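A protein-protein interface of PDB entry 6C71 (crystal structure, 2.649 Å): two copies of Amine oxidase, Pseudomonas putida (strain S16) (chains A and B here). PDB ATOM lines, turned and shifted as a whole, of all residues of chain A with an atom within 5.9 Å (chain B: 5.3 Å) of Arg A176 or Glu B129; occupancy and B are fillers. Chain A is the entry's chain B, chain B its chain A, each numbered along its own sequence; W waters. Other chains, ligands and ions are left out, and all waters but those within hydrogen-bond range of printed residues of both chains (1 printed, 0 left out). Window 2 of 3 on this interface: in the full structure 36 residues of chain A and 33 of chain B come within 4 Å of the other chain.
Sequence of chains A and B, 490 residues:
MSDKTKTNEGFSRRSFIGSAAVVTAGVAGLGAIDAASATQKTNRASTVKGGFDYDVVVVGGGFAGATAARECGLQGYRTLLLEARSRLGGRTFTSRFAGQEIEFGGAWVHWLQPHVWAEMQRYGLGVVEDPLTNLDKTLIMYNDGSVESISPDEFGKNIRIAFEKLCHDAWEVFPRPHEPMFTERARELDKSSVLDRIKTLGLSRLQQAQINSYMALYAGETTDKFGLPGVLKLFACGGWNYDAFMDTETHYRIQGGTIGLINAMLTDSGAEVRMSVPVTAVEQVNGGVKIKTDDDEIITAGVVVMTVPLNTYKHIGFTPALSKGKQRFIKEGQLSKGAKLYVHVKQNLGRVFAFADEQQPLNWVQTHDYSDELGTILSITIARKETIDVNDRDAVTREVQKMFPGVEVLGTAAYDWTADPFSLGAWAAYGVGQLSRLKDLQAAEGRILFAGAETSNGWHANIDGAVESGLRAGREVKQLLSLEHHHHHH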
ATOM      1  N   PHE A 174      -0.417 -16.029 -12.781  1.00  0.00           N
ATOM      2  CA  PHE A 174      -1.277 -16.749 -13.721  1.00  0.00           C
ATOM      3  C   PHE A 174      -2.124 -17.795 -13.003  1.00  0.00           C
ATOM      4  O   PHE A 174      -1.889 -19.002 -13.141  1.00  0.00           O
ATOM      5  CB  PHE A 174      -0.448 -17.405 -14.827  1.00  0.00           C
ATOM      6  CG  PHE A 174       0.182 -16.428 -15.778  1.00  0.00           C
ATOM      7  CD1 PHE A 174       1.531 -16.128 -15.688  1.00  0.00           C
ATOM      8  CD2 PHE A 174      -0.569 -15.825 -16.774  1.00  0.00           C
ATOM      9  CE1 PHE A 174       2.117 -15.235 -16.566  1.00  0.00           C
ATOM     10  CE2 PHE A 174       0.011 -14.930 -17.654  1.00  0.00           C
ATOM     11  CZ  PHE A 174       1.356 -14.635 -17.549  1.00  0.00           C
ATOM     12  N   PRO A 175      -3.124 -17.367 -12.228  1.00  0.00           N
ATOM     13  CA  PRO A 175      -4.084 -18.343 -11.693  1.00  0.00           C
ATOM     14  C   PRO A 175      -4.949 -18.968 -12.774  1.00  0.00           C
ATOM     15  O   PRO A 175      -5.444 -20.086 -12.587  1.00  0.00           O
ATOM     16  CB  PRO A 175      -4.918 -17.514 -10.706  1.00  0.00           C
ATOM     17  CG  PRO A 175      -4.822 -16.123 -11.219  1.00  0.00           C
ATOM     18  CD  PRO A 175      -3.441 -15.994 -11.803  1.00  0.00           C
ATOM     19  N   ARG A 176      -5.150 -18.276 -13.897  1.00  0.00           N
ATOM     20  CA  ARG A 176      -5.892 -18.790 -15.048  1.00  0.00           C
ATOM     21  C   ARG A 176      -4.988 -18.696 -16.269  1.00  0.00           C
ATOM     22  O   ARG A 176      -5.005 -17.683 -16.988  1.00  0.00           O
ATOM     23  CB  ARG A 176      -7.188 -18.014 -15.268  1.00  0.00           C
ATOM     24  CG  ARG A 176      -8.098 -17.926 -14.056  1.00  0.00           C
ATOM     25  CD  ARG A 176      -9.415 -17.281 -14.450  1.00  0.00           C
ATOM     26  NE  ARG A 176     -10.230 -16.891 -13.305  1.00  0.00           N
ATOM     27  CZ  ARG A 176     -11.444 -16.358 -13.409  1.00  0.00           C
ATOM     28  NH1 ARG A 176     -11.977 -16.156 -14.606  1.00  0.00           N
ATOM     29  NH2 ARG A 176     -12.127 -16.028 -12.321  1.00  0.00           N
ATOM     30  N   PRO A 177      -4.182 -19.722 -16.543  1.00  0.00           N
ATOM     31  CA  PRO A 177      -3.234 -19.631 -17.665  1.00  0.00           C
ATOM     32  C   PRO A 177      -3.888 -19.430 -19.025  1.00  0.00           C
ATOM     33  O   PRO A 177      -3.227 -18.917 -19.936  1.00  0.00           O
ATOM     34  CB  PRO A 177      -2.485 -20.971 -17.602  1.00  0.00           C
ATOM     35  CG  PRO A 177      -2.718 -21.493 -16.223  1.00  0.00           C
ATOM     36  CD  PRO A 177      -4.073 -21.006 -15.828  1.00  0.00           C
ATOM     37  N   HIS A 178      -5.149 -19.818 -19.203  1.00  0.00           N
ATOM     38  CA  HIS A 178      -5.831 -19.668 -20.482  1.00  0.00           C
ATOM     39  C   HIS A 178      -6.538 -18.336 -20.637  1.00  0.00           C
ATOM     40  O   HIS A 178      -7.181 -18.106 -21.668  1.00  0.00           O
ATOM     41  CB  HIS A 178      -6.823 -20.823 -20.686  1.00  0.00           C
ATOM     42  CG  HIS A 178      -6.158 -22.134 -20.973  1.00  0.00           C
ATOM     43  ND1 HIS A 178      -5.667 -22.960 -19.983  1.00  0.00           N
ATOM     44  CD2 HIS A 178      -5.888 -22.749 -22.147  1.00  0.00           C
ATOM     45  CE1 HIS A 178      -5.140 -24.037 -20.538  1.00  0.00           C
ATOM     46  NE2 HIS A 178      -5.259 -23.931 -21.850  1.00  0.00           N
ATOM     47  N   GLU A 179      -6.435 -17.458 -19.643  1.00  0.00           N
ATOM     48  CA  GLU A 179      -6.749 -16.040 -19.775  1.00  0.00           C
ATOM     49  C   GLU A 179      -5.489 -15.285 -19.343  1.00  0.00           C
ATOM     50  O   GLU A 179      -5.364 -14.868 -18.177  1.00  0.00           O
ATOM     51  CB  GLU A 179      -7.972 -15.663 -18.949  1.00  0.00           C
ATOM     52  CG  GLU A 179      -9.059 -16.721 -19.016  1.00  0.00           C
ATOM     53  CD  GLU A 179     -10.226 -16.455 -18.078  1.00  0.00           C
ATOM     54  OE1 GLU A 179     -10.683 -15.300 -18.010  1.00  0.00           O
ATOM     55  OE2 GLU A 179     -10.676 -17.416 -17.412  1.00  0.00           O
ATOM     56  N   PRO A 180      -4.533 -15.093 -20.263  1.00  0.00           N
ATOM     57  CA  PRO A 180      -3.203 -14.634 -19.850  1.00  0.00           C
ATOM     58  C   PRO A 180      -3.172 -13.264 -19.219  1.00  0.00           C
ATOM     59  O   PRO A 180      -2.334 -13.036 -18.341  1.00  0.00           O
ATOM     60  CB  PRO A 180      -2.397 -14.678 -21.168  1.00  0.00           C
ATOM     61  CG  PRO A 180      -3.136 -15.604 -22.052  1.00  0.00           C
ATOM     62  CD  PRO A 180      -4.595 -15.357 -21.710  1.00  0.00           C
ATOM     63  N   PHE A 182      -5.360 -11.964 -17.179  1.00  0.00           N
ATOM     64  CA  PHE A 182      -6.352 -11.938 -16.109  1.00  0.00           C
ATOM     65  C   PHE A 182      -5.897 -11.062 -14.936  1.00  0.00           C
ATOM     66  O   PHE A 182      -6.674 -10.248 -14.433  1.00  0.00           O
ATOM     67  CB  PHE A 182      -6.665 -13.368 -15.656  1.00  0.00           C
ATOM     68  CG  PHE A 182      -7.702 -13.447 -14.574  1.00  0.00           C
ATOM     69  CD1 PHE A 182      -9.035 -13.177 -14.844  1.00  0.00           C
ATOM     70  CD2 PHE A 182      -7.339 -13.767 -13.278  1.00  0.00           C
ATOM     71  CE1 PHE A 182      -9.988 -13.245 -13.843  1.00  0.00           C
ATOM     72  CE2 PHE A 182      -8.286 -13.833 -12.271  1.00  0.00           C
ATOM     73  CZ  PHE A 182      -9.613 -13.572 -12.555  1.00  0.00           C
ATOM     74  N   TRP A 240       1.615 -25.608 -12.648  1.00  0.00           N
ATOM     75  CA  TRP A 240       2.431 -24.815 -11.726  1.00  0.00           C
ATOM     76  C   TRP A 240       3.499 -25.660 -11.037  1.00  0.00           C
ATOM     77  O   TRP A 240       3.955 -25.324  -9.941  1.00  0.00           O
ATOM     78  CB  TRP A 240       1.574 -24.112 -10.667  1.00  0.00           C
ATOM     79  CG  TRP A 240       0.470 -23.260 -11.201  1.00  0.00           C
ATOM     80  CD1 TRP A 240       0.567 -21.977 -11.655  1.00  0.00           C
ATOM     81  CD2 TRP A 240      -0.913 -23.619 -11.306  1.00  0.00           C
ATOM     82  NE1 TRP A 240      -0.667 -21.521 -12.049  1.00  0.00           N
ATOM     83  CE2 TRP A 240      -1.592 -22.510 -11.844  1.00  0.00           C
ATOM     84  CE3 TRP A 240      -1.639 -24.775 -11.004  1.00  0.00           C
ATOM     85  CZ2 TRP A 240      -2.965 -22.521 -12.087  1.00  0.00           C
ATOM     86  CZ3 TRP A 240      -3.002 -24.785 -11.245  1.00  0.00           C
ATOM     87  CH2 TRP A 240      -3.650 -23.665 -11.782  1.00  0.00           C
ATOM     88  N   TRP B 111      -8.972 -26.755 -16.560  1.00  0.00           N
ATOM     89  CA  TRP B 111      -8.237 -26.857 -17.815  1.00  0.00           C
ATOM     90  C   TRP B 111      -7.223 -27.993 -17.824  1.00  0.00           C
ATOM     91  O   TRP B 111      -6.722 -28.342 -18.899  1.00  0.00           O
ATOM     92  CB  TRP B 111      -7.531 -25.534 -18.134  1.00  0.00           C
ATOM     93  CG  TRP B 111      -6.801 -24.931 -16.979  1.00  0.00           C
ATOM     94  CD1 TRP B 111      -5.500 -25.142 -16.629  1.00  0.00           C
ATOM     95  CD2 TRP B 111      -7.327 -24.002 -16.023  1.00  0.00           C
ATOM     96  NE1 TRP B 111      -5.184 -24.406 -15.512  1.00  0.00           N
ATOM     97  CE2 TRP B 111      -6.289 -23.698 -15.121  1.00  0.00           C
ATOM     98  CE3 TRP B 111      -8.576 -23.400 -15.843  1.00  0.00           C
ATOM     99  CZ2 TRP B 111      -6.462 -22.820 -14.053  1.00  0.00           C
ATOM    100  CZ3 TRP B 111      -8.745 -22.528 -14.783  1.00  0.00           C
ATOM    101  CH2 TRP B 111      -7.694 -22.246 -13.903  1.00  0.00           C
ATOM    102  N   VAL B 127     -15.189 -19.781 -17.589  1.00  0.00           N
ATOM    103  CA  VAL B 127     -15.322 -20.338 -16.251  1.00  0.00           C
ATOM    104  C   VAL B 127     -15.966 -19.308 -15.332  1.00  0.00           C
ATOM    105  O   VAL B 127     -15.943 -18.102 -15.585  1.00  0.00           O
ATOM    106  CB  VAL B 127     -13.971 -20.810 -15.672  1.00  0.00           C
ATOM    107  CG1 VAL B 127     -13.384 -21.922 -16.526  1.00  0.00           C
ATOM    108  CG2 VAL B 127     -12.999 -19.643 -15.565  1.00  0.00           C
ATOM    109  N   VAL B 128     -16.546 -19.813 -14.247  1.00  0.00           N
ATOM    110  CA  VAL B 128     -17.052 -19.003 -13.148  1.00  0.00           C
ATOM    111  C   VAL B 128     -16.321 -19.447 -11.892  1.00  0.00           C
ATOM    112  O   VAL B 128     -16.393 -20.621 -11.511  1.00  0.00           O
ATOM    113  CB  VAL B 128     -18.573 -19.155 -12.980  1.00  0.00           C
ATOM    114  CG1 VAL B 128     -19.003 -18.729 -11.584  1.00  0.00           C
ATOM    115  CG2 VAL B 128     -19.307 -18.356 -14.042  1.00  0.00           C
ATOM    116  N   GLU B 129     -15.617 -18.521 -11.249  1.00  0.00           N
ATOM    117  CA  GLU B 129     -14.806 -18.864 -10.090  1.00  0.00           C
ATOM    118  C   GLU B 129     -15.669 -18.839  -8.837  1.00  0.00           C
ATOM    119  O   GLU B 129     -16.408 -17.877  -8.603  1.00  0.00           O
ATOM    120  CB  GLU B 129     -13.622 -17.912  -9.935  1.00  0.00           C
ATOM    121  CG  GLU B 129     -12.894 -18.075  -8.606  1.00  0.00           C
ATOM    122  CD  GLU B 129     -11.568 -17.344  -8.559  1.00  0.00           C
ATOM    123  OE1 GLU B 129     -10.744 -17.670  -7.678  1.00  0.00           O
ATOM    124  OE2 GLU B 129     -11.345 -16.451  -9.403  1.00  0.00           O
ATOM    125  N   ASP B 130     -15.580 -19.887  -8.051  1.00  0.00           N
ATOM    126  CA  ASP B 130     -16.266 -19.920  -6.771  1.00  0.00           C
ATOM    127  C   ASP B 130     -15.324 -19.443  -5.667  1.00  0.00           C
ATOM    128  O   ASP B 130     -14.103 -19.595  -5.780  1.00  0.00           O
ATOM    129  CB  ASP B 130     -16.761 -21.334  -6.473  1.00  0.00           C
ATOM    130  CG  ASP B 130     -18.116 -21.616  -7.097  1.00  0.00           C
ATOM    131  OD1 ASP B 130     -18.838 -20.647  -7.409  1.00  0.00           O
ATOM    132  OD2 ASP B 130     -18.456 -22.806  -7.277  1.00  0.00           O
ATOM    133  N   PRO B 131     -15.846 -18.864  -4.578  1.00  0.00           N
ATOM    134  CA  PRO B 131     -14.951 -18.240  -3.592  1.00  0.00           C
ATOM    135  C   PRO B 131     -14.207 -19.274  -2.763  1.00  0.00           C
ATOM    136  O   PRO B 131     -14.584 -19.558  -1.621  1.00  0.00           O
ATOM    137  CB  PRO B 131     -15.898 -17.396  -2.731  1.00  0.00           C
ATOM    138  CG  PRO B 131     -17.276 -17.943  -2.970  1.00  0.00           C
ATOM    139  CD  PRO B 131     -17.241 -18.923  -4.105  1.00  0.00           C
ATOM    140  N   THR B 133     -10.503 -19.235  -2.675  1.00  0.00           N
ATOM    141  CA  THR B 133      -9.251 -18.660  -2.207  1.00  0.00           C
ATOM    142  C   THR B 133      -9.523 -17.573  -1.173  1.00  0.00           C
ATOM    143  O   THR B 133     -10.621 -17.017  -1.099  1.00  0.00           O
ATOM    144  CB  THR B 133      -8.446 -18.086  -3.377  1.00  0.00           C
ATOM    145  OG1 THR B 133      -9.113 -16.930  -3.897  1.00  0.00           O
ATOM    146  CG2 THR B 133      -8.307 -19.123  -4.482  1.00  0.00           C
ATOM    147  N   HIS B 251     -13.184 -25.514  -7.735  1.00  0.00           N
ATOM    148  CA  HIS B 251     -12.894 -24.092  -7.883  1.00  0.00           C
ATOM    149  C   HIS B 251     -13.718 -23.419  -8.976  1.00  0.00           C
ATOM    150  O   HIS B 251     -14.298 -22.355  -8.742  1.00  0.00           O
ATOM    151  CB  HIS B 251     -11.397 -23.887  -8.150  1.00  0.00           C
ATOM    152  CG  HIS B 251     -10.909 -22.508  -7.828  1.00  0.00           C
ATOM    153  ND1 HIS B 251      -9.582 -22.147  -7.924  1.00  0.00           N
ATOM    154  CD2 HIS B 251     -11.570 -21.399  -7.419  1.00  0.00           C
ATOM    155  CE1 HIS B 251      -9.447 -20.878  -7.583  1.00  0.00           C
ATOM    156  NE2 HIS B 251     -10.639 -20.401  -7.274  1.00  0.00           N
ATOM    157  N   TYR B 252     -13.777 -24.007 -10.171  1.00  0.00           N
ATOM    158  CA  TYR B 252     -14.355 -23.346 -11.335  1.00  0.00           C
ATOM    159  C   TYR B 252     -15.542 -24.125 -11.883  1.00  0.00           C
ATOM    160  O   TYR B 252     -15.443 -25.331 -12.130  1.00  0.00           O
ATOM    161  CB  TYR B 252     -13.306 -23.168 -12.434  1.00  0.00           C
ATOM    162  CG  TYR B 252     -12.104 -22.371 -11.997  1.00  0.00           C
ATOM    163  CD1 TYR B 252     -12.126 -20.983 -12.012  1.00  0.00           C
ATOM    164  CD2 TYR B 252     -10.945 -23.004 -11.570  1.00  0.00           C
ATOM    165  CE1 TYR B 252     -11.027 -20.248 -11.614  1.00  0.00           C
ATOM    166  CE2 TYR B 252      -9.842 -22.277 -11.170  1.00  0.00           C
ATOM    167  CZ  TYR B 252      -9.888 -20.900 -11.194  1.00  0.00           C
ATOM    168  OH  TYR B 252      -8.791 -20.169 -10.796  1.00  0.00           O
ATOM    169  N   ARG B 253     -16.647 -23.418 -12.095  1.00  0.00           N
ATOM    170  CA  ARG B 253     -17.838 -23.907 -12.772  1.00  0.00           C
ATOM    171  C   ARG B 253     -17.828 -23.464 -14.232  1.00  0.00           C
ATOM    172  O   ARG B 253     -17.034 -22.619 -14.647  1.00  0.00           O
ATOM    173  CB  ARG B 253     -19.096 -23.389 -12.063  1.00  0.00           C
ATOM    174  CG  ARG B 253     -19.187 -23.753 -10.590  1.00  0.00           C
ATOM    175  CD  ARG B 253     -20.528 -23.343  -9.987  1.00  0.00           C
ATOM    176  NE  ARG B 253     -20.614 -21.885  -9.891  1.00  0.00           N
ATOM    177  CZ  ARG B 253     -21.734 -21.174  -9.971  1.00  0.00           C
ATOM    178  NH1 ARG B 253     -22.901 -21.774 -10.163  1.00  0.00           N
ATOM    179  NH2 ARG B 253     -21.683 -19.854  -9.859  1.00  0.00           N
HETATM  180  O   HOH W   1     -13.332 -17.861 -18.360  1.00  0.00           O
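Among the printed residues, merely in contact across the chains: Pro A175 with Trp B111 (3.3 Å), Pro A177 with Trp B111 (3.5 Å), His A178 with Trp B111 (3.7 Å), Glu A179 with Val B127 (3.7 Å), Trp A240 with Trp B111 (3.7 Å), Arg A176 with Val B127 (3.8 Å), Pro A175 with Tyr B252 (3.8 Å) and Arg A176 with Tyr B252 (3.8 Å).
Water W1 bridges N of Val B127 (2.8 Å) and OE2 of Glu A179 (2.9 Å).
NE2 of His B251 lies within hydrogen-bond range of OE1 of Glu B129, at 2.8 Å. NE1 of Trp A240 sits at hydrogen-bond distance from O of Phe A174 (3.0 Å). The guanidinium group (NH1) of Arg A176 is in salt-bridge range of the side-chain carboxylate (OE2) of Glu A179 (3.3 Å).
The side-chain carboxylate (OE2) of Glu B129 lies within salt-bridge range of the guanidinium group (NH2) of Arg A176 (3.1 Å).
Printed residues of chain B that touch a printed residue of chain A: Trp B111, Val B127, Glu B129 and Tyr B252. Hydrophobic or aromatic side chains of chain B within 4 Å of the printed part of chain A: Trp B111, Val B127 and Tyr B252. Printed residues of chain A that touch a printed residue of chain B: Pro A175, Arg A176, Pro A177, His A178, Glu A179 and Trp A240. Hydrophobic or aromatic side chains of chain A that line the printed part of chain B: Pro A177, His A178 and Trp A240.
Of chain B, only Val B127, Glu B129 and Tyr B252 come within 4 Å of Arg A176. Of the printed residues of chain A, Glu B129 touches Arg A176 (3.1 Å). Of the printed residues of chain B, Glu A179 touches Val B127. Of the printed residues of chain B, Trp A240 touches Trp B111 (3.7 Å). His B251 touches none of the printed residues of chain A. Pro B131 touches none of the printed residues of chain A. The nearest printed residue of chain A that does not touch Val B127 is Phe A182 (7.3 Å).
No position is printed for both chains. Of the 9 pairs that touch across the chains among the printed residues, none has its exchanged pair printed and touching as well.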
